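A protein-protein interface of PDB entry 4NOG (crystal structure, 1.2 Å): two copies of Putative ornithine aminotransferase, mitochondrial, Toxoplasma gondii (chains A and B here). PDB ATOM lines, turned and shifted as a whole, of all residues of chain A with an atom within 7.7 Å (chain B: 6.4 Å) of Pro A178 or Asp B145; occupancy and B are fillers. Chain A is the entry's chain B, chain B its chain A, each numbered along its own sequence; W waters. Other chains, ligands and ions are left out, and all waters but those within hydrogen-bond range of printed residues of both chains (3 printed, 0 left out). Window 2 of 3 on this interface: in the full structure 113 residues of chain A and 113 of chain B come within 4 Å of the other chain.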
ATOM      1  N   ILE A 161     -25.182 -22.172  17.876  1.00  0.00           N
ATOM      2  CA  ILE A 161     -23.900 -22.119  18.563  1.00  0.00           C
ATOM      3  C   ILE A 161     -23.733 -23.246  19.555  1.00  0.00           C
ATOM      4  O   ILE A 161     -22.634 -23.767  19.690  1.00  0.00           O
ATOM      5  CB  ILE A 161     -23.662 -20.718  19.132  1.00  0.00           C
ATOM      6  CG1 ILE A 161     -23.401 -19.730  17.988  1.00  0.00           C
ATOM      7  CG2 ILE A 161     -22.568 -20.730  20.168  1.00  0.00           C
ATOM      8  CD1 ILE A 161     -23.553 -18.272  18.404  1.00  0.00           C
ATOM      9  N   THR A 162     -24.793 -23.607  20.273  1.00  0.00           N
ATOM     10  CA  THR A 162     -24.679 -24.713  21.222  1.00  0.00           C
ATOM     11  C   THR A 162     -24.395 -26.068  20.500  1.00  0.00           C
ATOM     12  O   THR A 162     -23.639 -26.899  21.005  1.00  0.00           O
ATOM     13  CB  THR A 162     -25.831 -24.706  22.200  1.00  0.00           C
ATOM     14  OG1 THR A 162     -25.787 -23.468  22.969  1.00  0.00           O
ATOM     15  CG2 THR A 162     -25.750 -25.876  23.195  1.00  0.00           C
ATOM     16  N   SER A 165     -20.806 -26.036  19.620  1.00  0.00           N
ATOM     17  CA  SER A 165     -20.057 -26.195  20.876  1.00  0.00           C
ATOM     18  C   SER A 165     -19.952 -27.633  21.304  1.00  0.00           C
ATOM     19  O   SER A 165     -19.164 -27.924  22.219  1.00  0.00           O
ATOM     20  CB  SER A 165     -20.792 -25.445  22.008  1.00  0.00           C
ATOM     21  OG  SER A 165     -20.870 -24.045  21.691  1.00  0.00           O
ATOM     22  N   TYR A 173     -17.426 -26.024  13.971  1.00  0.00           N
ATOM     23  CA  TYR A 173     -17.144 -25.173  15.124  1.00  0.00           C
ATOM     24  C   TYR A 173     -16.151 -24.040  14.902  1.00  0.00           C
ATOM     25  O   TYR A 173     -16.153 -23.082  15.666  1.00  0.00           O
ATOM     26  CB  TYR A 173     -16.724 -25.979  16.357  1.00  0.00           C
ATOM     27  CG  TYR A 173     -15.467 -26.783  16.231  1.00  0.00           C
ATOM     28  CD1 TYR A 173     -14.227 -26.164  16.364  1.00  0.00           C
ATOM     29  CD2 TYR A 173     -15.498 -28.150  16.009  1.00  0.00           C
ATOM     30  CE1 TYR A 173     -13.064 -26.908  16.241  1.00  0.00           C
ATOM     31  CE2 TYR A 173     -14.322 -28.885  15.927  1.00  0.00           C
ATOM     32  CZ  TYR A 173     -13.134 -28.262  16.074  1.00  0.00           C
ATOM     33  OH  TYR A 173     -11.976 -28.997  15.956  1.00  0.00           O
ATOM     34  N   ASN A 175     -13.976 -21.005  14.581  1.00  0.00           N
ATOM     35  CA  ASN A 175     -14.177 -19.556  14.626  1.00  0.00           C
ATOM     36  C   ASN A 175     -15.592 -19.145  14.902  1.00  0.00           C
ATOM     37  O   ASN A 175     -15.999 -18.050  14.577  1.00  0.00           O
ATOM     38  CB  ASN A 175     -13.655 -18.895  13.328  1.00  0.00           C
ATOM     39  CG  ASN A 175     -12.178 -18.664  13.350  1.00  0.00           C
ATOM     40  OD1 ASN A 175     -11.556 -18.627  14.333  1.00  0.00           O
ATOM     41  ND2 ASN A 175     -11.651 -18.458  12.191  1.00  0.00           N
ATOM     42  N   PHE A 176     -16.362 -20.013  15.570  1.00  0.00           N
ATOM     43  CA  PHE A 176     -17.707 -19.657  16.040  1.00  0.00           C
ATOM     44  C   PHE A 176     -17.835 -19.528  17.577  1.00  0.00           C
ATOM     45  O   PHE A 176     -18.937 -19.347  18.073  1.00  0.00           O
ATOM     46  CB  PHE A 176     -18.756 -20.652  15.540  1.00  0.00           C
ATOM     47  CG  PHE A 176     -18.940 -20.667  14.054  1.00  0.00           C
ATOM     48  CD1 PHE A 176     -19.198 -19.495  13.326  1.00  0.00           C
ATOM     49  CD2 PHE A 176     -18.863 -21.849  13.344  1.00  0.00           C
ATOM     50  CE1 PHE A 176     -19.398 -19.535  11.952  1.00  0.00           C
ATOM     51  CE2 PHE A 176     -19.062 -21.875  11.973  1.00  0.00           C
ATOM     52  CZ  PHE A 176     -19.312 -20.726  11.271  1.00  0.00           C
ATOM     53  N   GLY A 177     -16.712 -19.636  18.281  1.00  0.00           N
ATOM     54  CA  GLY A 177     -16.733 -19.530  19.731  1.00  0.00           C
ATOM     55  C   GLY A 177     -16.684 -18.094  20.211  1.00  0.00           C
ATOM     56  O   GLY A 177     -16.614 -17.126  19.412  1.00  0.00           O
ATOM     57  N   PRO A 178     -16.681 -17.896  21.511  1.00  0.00           N
ATOM     58  CA  PRO A 178     -16.540 -18.978  22.529  1.00  0.00           C
ATOM     59  C   PRO A 178     -17.779 -19.845  22.728  1.00  0.00           C
ATOM     60  O   PRO A 178     -18.903 -19.482  22.410  1.00  0.00           O
ATOM     61  CB  PRO A 178     -16.247 -18.166  23.806  1.00  0.00           C
ATOM     62  CG  PRO A 178     -16.955 -16.832  23.583  1.00  0.00           C
ATOM     63  CD  PRO A 178     -16.715 -16.562  22.116  1.00  0.00           C
ATOM     64  N   PHE A 179     -17.525 -21.050  23.218  1.00  0.00           N
ATOM     65  CA  PHE A 179     -18.482 -22.133  23.120  1.00  0.00           C
ATOM     66  C   PHE A 179     -19.271 -22.368  24.420  1.00  0.00           C
ATOM     67  O   PHE A 179     -18.787 -22.077  25.528  1.00  0.00           O
ATOM     68  CB  PHE A 179     -17.726 -23.387  22.742  1.00  0.00           C
ATOM     69  CG  PHE A 179     -17.063 -23.268  21.395  1.00  0.00           C
ATOM     70  CD1 PHE A 179     -17.845 -23.203  20.250  1.00  0.00           C
ATOM     71  CD2 PHE A 179     -15.683 -23.175  21.259  1.00  0.00           C
ATOM     72  CE1 PHE A 179     -17.260 -23.060  19.012  1.00  0.00           C
ATOM     73  CE2 PHE A 179     -15.063 -23.037  19.991  1.00  0.00           C
ATOM     74  CZ  PHE A 179     -15.874 -22.964  18.885  1.00  0.00           C
ATOM     75  N   THR A 180     -20.501 -22.854  24.257  1.00  0.00           N
ATOM     76  CA  THR A 180     -21.276 -23.262  25.399  1.00  0.00           C
ATOM     77  C   THR A 180     -20.588 -24.411  26.121  1.00  0.00           C
ATOM     78  O   THR A 180     -20.260 -25.406  25.462  1.00  0.00           O
ATOM     79  CB  THR A 180     -22.669 -23.770  24.956  1.00  0.00           C
ATOM     80  OG1 THR A 180     -23.238 -22.816  23.995  1.00  0.00           O
ATOM     81  CG2 THR A 180     -23.587 -23.992  26.117  1.00  0.00           C
ATOM     82  N   PRO A 181     -20.337 -24.263  27.428  1.00  0.00           N
ATOM     83  CA  PRO A 181     -19.746 -25.385  28.201  1.00  0.00           C
ATOM     84  C   PRO A 181     -20.784 -26.478  28.482  1.00  0.00           C
ATOM     85  O   PRO A 181     -21.973 -26.291  28.226  1.00  0.00           O
ATOM     86  CB  PRO A 181     -19.338 -24.740  29.552  1.00  0.00           C
ATOM     87  CG  PRO A 181     -19.730 -23.364  29.488  1.00  0.00           C
ATOM     88  CD  PRO A 181     -20.582 -23.081  28.308  1.00  0.00           C
ATOM     89  N   ARG B 133     -19.081 -13.357  14.715  1.00  0.00           N
ATOM     90  CA  ARG B 133     -17.902 -13.933  15.378  1.00  0.00           C
ATOM     91  C   ARG B 133     -16.819 -14.300  14.368  1.00  0.00           C
ATOM     92  O   ARG B 133     -15.653 -13.936  14.519  1.00  0.00           O
ATOM     93  CB  ARG B 133     -18.279 -15.089  16.260  1.00  0.00           C
ATOM     94  CG  ARG B 133     -19.038 -14.743  17.519  1.00  0.00           C
ATOM     95  CD  ARG B 133     -19.527 -16.021  18.226  1.00  0.00           C
ATOM     96  NE  ARG B 133     -19.931 -15.694  19.579  1.00  0.00           N
ATOM     97  CZ  ARG B 133     -20.050 -16.609  20.542  1.00  0.00           C
ATOM     98  NH1 ARG B 133     -19.965 -17.936  20.292  1.00  0.00           N
ATOM     99  NH2 ARG B 133     -20.335 -16.214  21.779  1.00  0.00           N
ATOM    100  N   TYR B 137     -12.999 -12.776  13.929  1.00  0.00           N
ATOM    101  CA  TYR B 137     -11.764 -13.516  13.953  1.00  0.00           C
ATOM    102  C   TYR B 137     -10.936 -13.394  12.703  1.00  0.00           C
ATOM    103  O   TYR B 137      -9.724 -13.279  12.775  1.00  0.00           O
ATOM    104  CB  TYR B 137     -12.032 -15.000  14.275  1.00  0.00           C
ATOM    105  CG  TYR B 137     -12.639 -15.225  15.671  1.00  0.00           C
ATOM    106  CD1 TYR B 137     -12.064 -14.672  16.810  1.00  0.00           C
ATOM    107  CD2 TYR B 137     -13.820 -15.958  15.854  1.00  0.00           C
ATOM    108  CE1 TYR B 137     -12.660 -14.830  18.056  1.00  0.00           C
ATOM    109  CE2 TYR B 137     -14.437 -16.095  17.100  1.00  0.00           C
ATOM    110  CZ  TYR B 137     -13.814 -15.555  18.182  1.00  0.00           C
ATOM    111  OH  TYR B 137     -14.344 -15.674  19.431  1.00  0.00           O
ATOM    112  N   ILE B 142      -9.217 -10.473  15.735  1.00  0.00           N
ATOM    113  CA  ILE B 142      -9.208 -10.483  17.204  1.00  0.00           C
ATOM    114  C   ILE B 142      -8.756 -11.839  17.718  1.00  0.00           C
ATOM    115  O   ILE B 142      -8.825 -12.835  16.981  1.00  0.00           O
ATOM    116  CB  ILE B 142     -10.541 -10.061  17.821  1.00  0.00           C
ATOM    117  CG1 ILE B 142     -11.562 -11.092  17.563  1.00  0.00           C
ATOM    118  CG2 ILE B 142     -11.019  -8.682  17.346  1.00  0.00           C
ATOM    119  CD1 ILE B 142     -12.804 -10.861  18.394  1.00  0.00           C
ATOM    120  N   PRO B 143      -8.238 -11.880  18.944  1.00  0.00           N
ATOM    121  CA  PRO B 143      -7.705 -13.153  19.400  1.00  0.00           C
ATOM    122  C   PRO B 143      -8.711 -14.302  19.482  1.00  0.00           C
ATOM    123  O   PRO B 143      -9.864 -14.083  19.671  1.00  0.00           O
ATOM    124  CB  PRO B 143      -7.225 -12.819  20.832  1.00  0.00           C
ATOM    125  CG  PRO B 143      -7.016 -11.377  20.846  1.00  0.00           C
ATOM    126  CD  PRO B 143      -7.990 -10.793  19.897  1.00  0.00           C
ATOM    127  N   PRO B 144      -8.251 -15.548  19.270  1.00  0.00           N
ATOM    128  CA  PRO B 144      -9.148 -16.690  19.245  1.00  0.00           C
ATOM    129  C   PRO B 144     -10.043 -16.737  20.501  1.00  0.00           C
ATOM    130  O   PRO B 144      -9.554 -16.526  21.621  1.00  0.00           O
ATOM    131  CB  PRO B 144      -8.182 -17.890  19.155  1.00  0.00           C
ATOM    132  CG  PRO B 144      -6.976 -17.333  18.429  1.00  0.00           C
ATOM    133  CD  PRO B 144      -6.864 -15.903  18.946  1.00  0.00           C
ATOM    134  N   ASP B 145     -11.313 -17.030  20.298  1.00  0.00           N
ATOM    135  CA  ASP B 145     -12.313 -17.166  21.338  1.00  0.00           C
ATOM    136  C   ASP B 145     -12.627 -15.909  22.128  1.00  0.00           C
ATOM    137  O   ASP B 145     -13.399 -15.989  23.107  1.00  0.00           O
ATOM    138  CB  ASP B 145     -11.982 -18.306  22.331  1.00  0.00           C
ATOM    139  CG  ASP B 145     -12.794 -19.540  22.096  1.00  0.00           C
ATOM    140  OD1 ASP B 145     -13.494 -19.672  21.092  1.00  0.00           O
ATOM    141  OD2 ASP B 145     -12.746 -20.430  22.939  1.00  0.00           O
ATOM    142  N   SER B 146     -12.083 -14.755  21.712  1.00  0.00           N
ATOM    143  CA  SER B 146     -12.299 -13.536  22.465  1.00  0.00           C
ATOM    144  C   SER B 146     -13.459 -12.707  22.000  1.00  0.00           C
ATOM    145  O   SER B 146     -13.685 -11.650  22.593  1.00  0.00           O
ATOM    146  CB  SER B 146     -11.025 -12.682  22.370  1.00  0.00           C
ATOM    147  OG  SER B 146     -10.938 -11.968  21.112  1.00  0.00           O
ATOM    148  N   ALA B 147     -14.211 -13.115  20.982  1.00  0.00           N
ATOM    149  CA  ALA B 147     -15.207 -12.210  20.392  1.00  0.00           C
ATOM    150  C   ALA B 147     -16.283 -11.909  21.455  1.00  0.00           C
ATOM    151  O   ALA B 147     -16.740 -12.844  22.154  1.00  0.00           O
ATOM    152  CB  ALA B 147     -15.851 -12.837  19.211  1.00  0.00           C
ATOM    153  N   LYS B 148     -16.701 -10.653  21.558  1.00  0.00           N
ATOM    154  CA  LYS B 148     -17.775 -10.229  22.368  1.00  0.00           C
ATOM    155  C   LYS B 148     -18.910  -9.637  21.512  1.00  0.00           C
ATOM    156  O   LYS B 148     -18.635  -8.999  20.484  1.00  0.00           O
ATOM    157  CB  LYS B 148     -17.295  -9.196  23.378  1.00  0.00           C
ATOM    158  CG  LYS B 148     -16.194  -9.646  24.244  1.00  0.00           C
ATOM    159  CD  LYS B 148     -16.610 -10.753  25.180  1.00  0.00           C
ATOM    160  CE  LYS B 148     -15.494 -11.110  26.144  1.00  0.00           C
ATOM    161  NZ  LYS B 148     -14.188 -11.350  25.379  1.00  0.00           N
ATOM    162  N   THR B 180     -23.496 -19.908  27.287  1.00  0.00           N
ATOM    163  CA  THR B 180     -22.508 -19.506  26.250  1.00  0.00           C
ATOM    164  C   THR B 180     -21.854 -18.178  26.712  1.00  0.00           C
ATOM    165  O   THR B 180     -22.616 -17.230  26.967  1.00  0.00           O
ATOM    166  CB  THR B 180     -23.233 -19.232  24.945  1.00  0.00           C
ATOM    167  OG1 THR B 180     -24.047 -20.349  24.575  1.00  0.00           O
ATOM    168  CG2 THR B 180     -22.205 -18.966  23.814  1.00  0.00           C
ATOM    169  N   PRO B 181     -20.542 -18.083  26.782  1.00  0.00           N
ATOM    170  CA  PRO B 181     -19.900 -16.803  27.050  1.00  0.00           C
ATOM    171  C   PRO B 181     -19.926 -15.869  25.884  1.00  0.00           C
ATOM    172  O   PRO B 181     -20.269 -16.228  24.780  1.00  0.00           O
ATOM    173  CB  PRO B 181     -18.430 -17.191  27.399  1.00  0.00           C
ATOM    174  CG  PRO B 181     -18.343 -18.639  27.317  1.00  0.00           C
ATOM    175  CD  PRO B 181     -19.550 -19.157  26.614  1.00  0.00           C
ATOM    176  N   GLY B 182     -19.468 -14.649  26.190  1.00  0.00           N
ATOM    177  CA  GLY B 182     -19.144 -13.721  25.128  1.00  0.00           C
ATOM    178  C   GLY B 182     -20.141 -12.621  24.919  1.00  0.00           C
ATOM    179  O   GLY B 182     -20.139 -11.979  23.856  1.00  0.00           O
HETATM  180  O   HOH W   1     -11.847 -18.141  17.588  1.00  0.00           O
HETATM  181  O   HOH W   2     -14.823 -21.396  24.220  1.00  0.00           O
HETATM  182  O   HOH W   3     -13.864 -19.879  18.285  1.00  0.00           O
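NH1 of Arg B133 lies within hydrogen-bond range of O of Phe A176, at 2.8 Å. The guanidinium group (NH1) of Arg B133 lies within hydrogen-bond range of the backbone carbonyl oxygen (O) of Pro A178 (2.8 Å). The side-chain hydroxyl (OH) of Tyr B137 is in hydrogen-bond range of the backbone carbonyl oxygen (O) of Gly A177 (2.7 Å). The side-chain hydroxyl (OG1) of Thr A180 lies within hydrogen-bond range of the side-chain hydroxyl (OG1) of Thr B180 (2.7 Å).
O of Pro B181 lies within hydrogen-bond range of NH2 of Arg B133 (3.0 Å). The backbone NH (N) of Asp B145 lies close to the side-chain hydroxyl (OH) of Tyr B137 (3.4 Å). The backbone NH (N) of Ser B146 sits at hydrogen-bond distance from the side-chain hydroxyl (OH) of Tyr B137, 3.3 Å away. The side-chain hydroxyl (OH) of Tyr B137 is in hydrogen-bond range of the backbone NH (N) of Ala B147, at 3.0 Å. The backbone carbonyl oxygen (O) of Ile A161 lies within hydrogen-bond range of the side-chain hydroxyl (OG) of Ser A165 (2.7 Å). The side-chain hydroxyl (OG) of Ser A165 sits at hydrogen-bond distance from the backbone NH (N) of Thr A180 (2.9 Å).
Thr A162 touches Thr B180. Asn A175 touches Arg B133 (O to C, 3.8 Å). Tyr B137 touches Asn A175 (CD2 to O, 3.3 Å). Gly A177 touches Arg B133 (C to NH1, 3.3 Å). Gly A177 touches Asp B145 (CA to OD1, 3.5 Å). Tyr B137 touches Pro A178 (OH to CD, 3.7 Å). Ala B147 touches Pro A178 (O to CD, 3.7 Å). Pro A178 touches Thr B180 (O to CG2, 3.6 Å). Pro A178 touches Pro B181 (CG to O, 3.6 Å). CE2 of Phe A179 touches OD1 of Asp B145 (3.9 Å).
Of the printed residues of chain B, Ile A161 touches Arg B133. Of the printed residues of chain B, Asn A175 touches Arg B133 and Tyr B137. Pro A178 touches six residues of chain B. Of the printed residues of chain B, Phe A179 touches Asp B145 and Pro B181. Ser B146 touches none of the printed residues of chain A. The nearest printed residue of chain A that does not touch Ala B147 is Gly A177 (4.4 Å).
Of the 11 printed residues of chain A, 8 touch a printed residue of chain B. Printed residues of chain A that touch a printed residue of chain B: Ile A161, Thr A162, Asn A175, Phe A176, Gly A177, Pro A178, Phe A179 and Thr A180. Hydrophobic or aromatic side chains of chain A that line the printed part of chain B: Ile A161, Pro A178 and Phe A179. Along chain A the printed residues that touch a printed residue of chain B span positions 161 to 180. Among the printed residues, no Asp or Glu carboxylate lies within 4 Å of a Lys or Arg side-chain nitrogen of the other chain.
Thr A180 touches its own counterpart, Thr B180. Positions printed for both chains: 180 and 181. Of the 17 pairs that touch across the chains among the printed residues, 1 has its exchanged pair printed and touching as well.
Water W2 bridges the side-chain carboxylate (OD2) of Asp B145 (2.6 Å) and the backbone NH (N) of Phe A179 (2.9 Å). Water W3 bridges the side-chain carboxylate (OD1) of Asp B145 (2.8 Å) and the backbone NH (N) of Gly A177 (2.9 Å). Water W1 bridges the backbone NH of Asp B145 (3.0 Å) and the side-chain amide oxygen of Asn A175 (3.3 Å).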
